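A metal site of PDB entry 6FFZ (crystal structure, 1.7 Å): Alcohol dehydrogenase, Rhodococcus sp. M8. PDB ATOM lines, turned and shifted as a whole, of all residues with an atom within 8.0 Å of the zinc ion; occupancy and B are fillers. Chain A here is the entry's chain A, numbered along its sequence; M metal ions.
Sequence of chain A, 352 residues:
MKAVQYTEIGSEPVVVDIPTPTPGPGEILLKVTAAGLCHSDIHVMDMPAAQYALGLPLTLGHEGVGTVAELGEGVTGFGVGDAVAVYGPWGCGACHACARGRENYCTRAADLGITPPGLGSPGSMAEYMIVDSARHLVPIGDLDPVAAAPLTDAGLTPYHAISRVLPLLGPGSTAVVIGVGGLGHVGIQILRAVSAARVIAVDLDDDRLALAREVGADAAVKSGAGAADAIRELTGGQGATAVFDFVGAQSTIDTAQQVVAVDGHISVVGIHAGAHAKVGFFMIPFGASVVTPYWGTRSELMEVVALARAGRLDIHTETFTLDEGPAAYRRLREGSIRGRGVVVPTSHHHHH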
ATOM      1  N   TRP A  90      27.417 -16.555   8.060  1.00  0.00           N
ATOM      2  CA  TRP A  90      27.709 -17.969   7.985  1.00  0.00           C
ATOM      3  C   TRP A  90      26.468 -18.796   8.234  1.00  0.00           C
ATOM      4  O   TRP A  90      25.699 -18.527   9.180  1.00  0.00           O
ATOM      5  CB  TRP A  90      28.799 -18.383   8.972  1.00  0.00           C
ATOM      6  CG  TRP A  90      30.143 -17.724   8.718  1.00  0.00           C
ATOM      7  CD1 TRP A  90      30.513 -16.973   7.634  1.00  0.00           C
ATOM      8  CD2 TRP A  90      31.289 -17.798   9.572  1.00  0.00           C
ATOM      9  NE1 TRP A  90      31.820 -16.549   7.770  1.00  0.00           N
ATOM     10  CE2 TRP A  90      32.321 -17.040   8.952  1.00  0.00           C
ATOM     11  CE3 TRP A  90      31.532 -18.387  10.809  1.00  0.00           C
ATOM     12  CZ2 TRP A  90      33.594 -16.885   9.518  1.00  0.00           C
ATOM     13  CZ3 TRP A  90      32.806 -18.231  11.395  1.00  0.00           C
ATOM     14  CH2 TRP A  90      33.807 -17.478  10.738  1.00  0.00           C
ATOM     15  N   GLY A  91      26.269 -19.779   7.360  1.00  0.00           N
ATOM     16  CA  GLY A  91      25.211 -20.753   7.515  1.00  0.00           C
ATOM     17  C   GLY A  91      25.736 -22.152   7.650  1.00  0.00           C
ATOM     18  O   GLY A  91      26.958 -22.383   7.687  1.00  0.00           O
ATOM     19  N   CYS A  92      24.803 -23.111   7.704  1.00  0.00           N
ATOM     20  CA  CYS A  92      25.137 -24.508   7.876  1.00  0.00           C
ATOM     21  C   CYS A  92      25.833 -25.116   6.643  1.00  0.00           C
ATOM     22  O   CYS A  92      26.509 -26.120   6.765  1.00  0.00           O
ATOM     23  CB  CYS A  92      23.918 -25.338   8.283  1.00  0.00           C
ATOM     24  SG  CYS A  92      22.715 -25.607   6.930  1.00  0.00           S
ATOM     25  N   GLY A  93      25.605 -24.531   5.485  1.00  0.00           N
ATOM     26  CA  GLY A  93      26.203 -25.012   4.228  1.00  0.00           C
ATOM     27  C   GLY A  93      25.431 -26.120   3.537  1.00  0.00           C
ATOM     28  O   GLY A  93      25.773 -26.488   2.390  1.00  0.00           O
ATOM     29  N   ALA A  94      24.395 -26.677   4.204  1.00  0.00           N
ATOM     30  CA  ALA A  94      23.761 -27.930   3.785  1.00  0.00           C
ATOM     31  C   ALA A  94      22.264 -27.837   3.464  1.00  0.00           C
ATOM     32  O   ALA A  94      21.747 -28.697   2.746  1.00  0.00           O
ATOM     33  CB  ALA A  94      23.964 -28.994   4.835  1.00  0.00           C
ATOM     34  N   CYS A  95      21.574 -26.874   4.056  1.00  0.00           N
ATOM     35  CA  CYS A  95      20.138 -26.704   3.839  1.00  0.00           C
ATOM     36  C   CYS A  95      19.843 -26.177   2.457  1.00  0.00           C
ATOM     37  O   CYS A  95      20.752 -25.808   1.696  1.00  0.00           O
ATOM     38  CB  CYS A  95      19.541 -25.764   4.915  1.00  0.00           C
ATOM     39  SG  CYS A  95      19.973 -24.041   4.758  1.00  0.00           S
ATOM     40  N   HIS A  96      18.575 -26.136   2.097  1.00  0.00           N
ATOM     41  CA  HIS A  96      18.184 -25.697   0.756  1.00  0.00           C
ATOM     42  C   HIS A  96      18.595 -24.267   0.427  1.00  0.00           C
ATOM     43  O   HIS A  96      19.070 -23.993  -0.685  1.00  0.00           O
ATOM     44  CB  HIS A  96      16.665 -25.916   0.604  1.00  0.00           C
ATOM     45  CG  HIS A  96      16.139 -25.618  -0.761  1.00  0.00           C
ATOM     46  ND1 HIS A  96      15.658 -24.377  -1.108  1.00  0.00           N
ATOM     47  CD2 HIS A  96      15.964 -26.403  -1.843  1.00  0.00           C
ATOM     48  CE1 HIS A  96      15.225 -24.413  -2.354  1.00  0.00           C
ATOM     49  NE2 HIS A  96      15.374 -25.639  -2.822  1.00  0.00           N
ATOM     50  N   ALA A  97      18.443 -23.340   1.374  1.00  0.00           N
ATOM     51  CA  ALA A  97      18.967 -22.010   1.218  1.00  0.00           C
ATOM     52  C   ALA A  97      20.487 -22.001   1.053  1.00  0.00           C
ATOM     53  O   ALA A  97      20.992 -21.369   0.110  1.00  0.00           O
ATOM     54  CB  ALA A  97      18.547 -21.123   2.390  1.00  0.00           C
ATOM     55  N   CYS A  98      21.217 -22.675   1.927  1.00  0.00           N
ATOM     56  CA  CYS A  98      22.675 -22.677   1.858  1.00  0.00           C
ATOM     57  C   CYS A  98      23.178 -23.327   0.562  1.00  0.00           C
ATOM     58  O   CYS A  98      24.184 -22.874   0.001  1.00  0.00           O
ATOM     59  CB  CYS A  98      23.321 -23.401   3.052  1.00  0.00           C
ATOM     60  SG  CYS A  98      23.238 -22.436   4.584  1.00  0.00           S
ATOM     61  N   ALA A  99      22.467 -24.350   0.086  1.00  0.00           N
ATOM     62  CA  ALA A  99      22.854 -25.013  -1.159  1.00  0.00           C
ATOM     63  C   ALA A  99      22.838 -24.053  -2.344  1.00  0.00           C
ATOM     64  O   ALA A  99      23.600 -24.243  -3.291  1.00  0.00           O
ATOM     65  CB  ALA A  99      21.995 -26.219  -1.418  1.00  0.00           C
ATOM     66  N   ARG A 102      22.679 -19.046  -0.281  1.00  0.00           N
ATOM     67  CA  ARG A 102      21.869 -18.038   0.421  1.00  0.00           C
ATOM     68  C   ARG A 102      21.984 -18.275   1.902  1.00  0.00           C
ATOM     69  O   ARG A 102      20.987 -18.502   2.608  1.00  0.00           O
ATOM     70  CB  ARG A 102      20.419 -18.089  -0.072  1.00  0.00           C
ATOM     71  CG  ARG A 102      20.299 -17.926  -1.591  1.00  0.00           C
ATOM     72  CD  ARG A 102      18.895 -18.190  -2.073  1.00  0.00           C
ATOM     73  NE  ARG A 102      17.918 -17.229  -1.556  1.00  0.00           N
ATOM     74  CZ  ARG A 102      17.727 -15.995  -2.058  1.00  0.00           C
ATOM     75  NH1 ARG A 102      18.471 -15.557  -3.068  1.00  0.00           N
ATOM     76  NH2 ARG A 102      16.818 -15.201  -1.523  1.00  0.00           N
ATOM     77  N   GLU A 103      23.218 -18.256   2.405  1.00  0.00           N
ATOM     78  CA  GLU A 103      23.464 -18.627   3.787  1.00  0.00           C
ATOM     79  C   GLU A 103      22.912 -17.593   4.757  1.00  0.00           C
ATOM     80  O   GLU A 103      22.657 -17.906   5.911  1.00  0.00           O
ATOM     81  CB  GLU A 103      24.954 -18.844   4.031  1.00  0.00           C
ATOM     82  CG  GLU A 103      25.524 -19.932   3.151  1.00  0.00           C
ATOM     83  CD  GLU A 103      26.805 -20.566   3.664  1.00  0.00           C
ATOM     84  OE1 GLU A 103      27.244 -20.264   4.794  1.00  0.00           O
ATOM     85  OE2 GLU A 103      27.349 -21.406   2.912  1.00  0.00           O
ATOM     86  N   ASN A 104      22.682 -16.380   4.249  1.00  0.00           N
ATOM     87  CA  ASN A 104      21.946 -15.360   4.994  1.00  0.00           C
ATOM     88  C   ASN A 104      20.537 -15.814   5.411  1.00  0.00           C
ATOM     89  O   ASN A 104      20.035 -15.381   6.450  1.00  0.00           O
ATOM     90  CB  ASN A 104      21.888 -14.031   4.237  1.00  0.00           C
ATOM     91  CG  ASN A 104      21.311 -14.151   2.835  1.00  0.00           C
ATOM     92  OD1 ASN A 104      21.528 -15.151   2.135  1.00  0.00           O
ATOM     93  ND2 ASN A 104      20.618 -13.101   2.391  1.00  0.00           N
ATOM     94  N   TYR A 105      19.943 -16.724   4.620  1.00  0.00           N
ATOM     95  CA  TYR A 105      18.609 -17.252   4.930  1.00  0.00           C
ATOM     96  C   TYR A 105      18.647 -18.701   5.391  1.00  0.00           C
ATOM     97  O   TYR A 105      17.652 -19.435   5.294  1.00  0.00           O
ATOM     98  CB  TYR A 105      17.674 -17.048   3.723  1.00  0.00           C
ATOM     99  CG  TYR A 105      17.465 -15.578   3.398  1.00  0.00           C
ATOM    100  CD1 TYR A 105      17.163 -14.628   4.408  1.00  0.00           C
ATOM    101  CD2 TYR A 105      17.564 -15.123   2.084  1.00  0.00           C
ATOM    102  CE1 TYR A 105      16.988 -13.303   4.093  1.00  0.00           C
ATOM    103  CE2 TYR A 105      17.367 -13.795   1.771  1.00  0.00           C
ATOM    104  CZ  TYR A 105      17.080 -12.878   2.800  1.00  0.00           C
ATOM    105  OH  TYR A 105      16.911 -11.545   2.495  1.00  0.00           O
ATOM    106  N   CYS A 106      19.790 -19.115   5.941  1.00  0.00           N
ATOM    107  CA  CYS A 106      19.932 -20.459   6.480  1.00  0.00           C
ATOM    108  C   CYS A 106      18.925 -20.707   7.589  1.00  0.00           C
ATOM    109  O   CYS A 106      18.798 -19.898   8.497  1.00  0.00           O
ATOM    110  CB  CYS A 106      21.330 -20.633   7.053  1.00  0.00           C
ATOM    111  SG  CYS A 106      21.602 -22.218   7.837  1.00  0.00           S
ATOM    112  N   THR A 107      18.225 -21.826   7.505  1.00  0.00           N
ATOM    113  CA  THR A 107      17.205 -22.235   8.478  1.00  0.00           C
ATOM    114  C   THR A 107      17.762 -23.033   9.662  1.00  0.00           C
ATOM    115  O   THR A 107      17.024 -23.398  10.559  1.00  0.00           O
ATOM    116  CB  THR A 107      16.142 -23.108   7.759  1.00  0.00           C
ATOM    117  OG1 THR A 107      16.805 -24.085   6.928  1.00  0.00           O
ATOM    118  CG2 THR A 107      15.280 -22.235   6.852  1.00  0.00           C
ATOM    119  N   ARG A 108      19.070 -23.313   9.673  1.00  0.00           N
ATOM    120  CA  ARG A 108      19.671 -24.154  10.702  1.00  0.00           C
ATOM    121  C   ARG A 108      20.713 -23.449  11.568  1.00  0.00           C
ATOM    122  O   ARG A 108      21.106 -23.990  12.580  1.00  0.00           O
ATOM    123  CB  ARG A 108      20.308 -25.379  10.050  1.00  0.00           C
ATOM    124  CG  ARG A 108      19.358 -26.217   9.219  1.00  0.00           C
ATOM    125  CD  ARG A 108      20.001 -27.561   8.941  1.00  0.00           C
ATOM    126  NE  ARG A 108      19.409 -28.236   7.773  1.00  0.00           N
ATOM    127  CZ  ARG A 108      20.013 -29.166   7.027  1.00  0.00           C
ATOM    128  NH1 ARG A 108      19.365 -29.670   5.981  1.00  0.00           N
ATOM    129  NH2 ARG A 108      21.267 -29.562   7.256  1.00  0.00           N
ATOM    130  N   ALA A 109      21.140 -22.267  11.163  1.00  0.00           N
ATOM    131  CA  ALA A 109      22.287 -21.617  11.810  1.00  0.00           C
ATOM    132  C   ALA A 109      22.024 -21.325  13.273  1.00  0.00           C
ATOM    133  O   ALA A 109      22.858 -21.636  14.120  1.00  0.00           O
ATOM    134  CB  ALA A 109      22.690 -20.363  11.054  1.00  0.00           C
ATOM    135  N   LEU A 112      22.096 -24.505  15.325  1.00  0.00           N
ATOM    136  CA  LEU A 112      23.459 -25.027  15.386  1.00  0.00           C
ATOM    137  C   LEU A 112      24.472 -24.084  16.089  1.00  0.00           C
ATOM    138  O   LEU A 112      25.643 -24.431  16.214  1.00  0.00           O
ATOM    139  CB  LEU A 112      23.942 -25.393  13.966  1.00  0.00           C
ATOM    140  CG  LEU A 112      23.189 -26.540  13.255  1.00  0.00           C
ATOM    141  CD1 LEU A 112      23.606 -26.610  11.783  1.00  0.00           C
ATOM    142  CD2 LEU A 112      23.408 -27.876  13.948  1.00  0.00           C
ATOM    143  N   ILE A 114      25.600 -21.177  14.861  1.00  0.00           N
ATOM    144  CA  ILE A 114      26.503 -20.653  13.865  1.00  0.00           C
ATOM    145  C   ILE A 114      26.239 -19.149  13.795  1.00  0.00           C
ATOM    146  O   ILE A 114      25.152 -18.709  13.440  1.00  0.00           O
ATOM    147  CB  ILE A 114      26.301 -21.287  12.471  1.00  0.00           C
ATOM    148  CG1 ILE A 114      26.635 -22.779  12.545  1.00  0.00           C
ATOM    149  CG2 ILE A 114      27.210 -20.626  11.432  1.00  0.00           C
ATOM    150  CD1 ILE A 114      26.242 -23.562  11.292  1.00  0.00           C
ATOM    151  N   ARG A 135      34.627 -21.832   1.824  1.00  0.00           N
ATOM    152  CA  ARG A 135      33.490 -21.266   1.089  1.00  0.00           C
ATOM    153  C   ARG A 135      33.097 -19.883   1.575  1.00  0.00           C
ATOM    154  O   ARG A 135      32.309 -19.210   0.927  1.00  0.00           O
ATOM    155  CB  ARG A 135      32.306 -22.235   1.135  1.00  0.00           C
ATOM    156  CG  ARG A 135      31.451 -22.174   2.384  1.00  0.00           C
ATOM    157  CD  ARG A 135      30.319 -23.199   2.347  1.00  0.00           C
ATOM    158  NE  ARG A 135      29.470 -23.016   3.512  1.00  0.00           N
ATOM    159  CZ  ARG A 135      29.675 -23.532   4.711  1.00  0.00           C
ATOM    160  NH1 ARG A 135      30.709 -24.335   4.958  1.00  0.00           N
ATOM    161  NH2 ARG A 135      28.820 -23.250   5.694  1.00  0.00           N
HETATM  162 ZN    ZN M   1      21.879 -23.666   6.057  1.00  0.00          ZN
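The side-chain sulfur (SG) of Cys 92 sits close to the backbone NH (N) of Ala 94 (3.4 Å). The side-chain sulfur (SG) of Cys 106 lies close to the backbone NH (N) of Arg 108 (3.3 Å). The side-chain sulfur of Cys 106 lies close to the backbone NH of Ala 109. SG of Cys 95 sits close to N of Ala 97 (3.8 Å). The side-chain sulfur (SG) of Cys 98 lies close to the backbone NH (N) of Gly 93 (3.3 Å).
Merely in contact with the zinc ion: Gly 93. Within 4 Å of the zinc ion: Cys 92, Gly 93, Cys 95, Cys 98 and Cys 106.
The zinc ion is bound by SG of Cys 92. The zinc ion is bound by SG of Cys 106 (2.3 Å). The zinc ion is bound by SG of Cys 95 (2.3 Å). The zinc ion is bound by the side-chain sulfur (SG) of Cys 98 (2.4 Å). The zinc ion has four donor atoms within binding distance.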
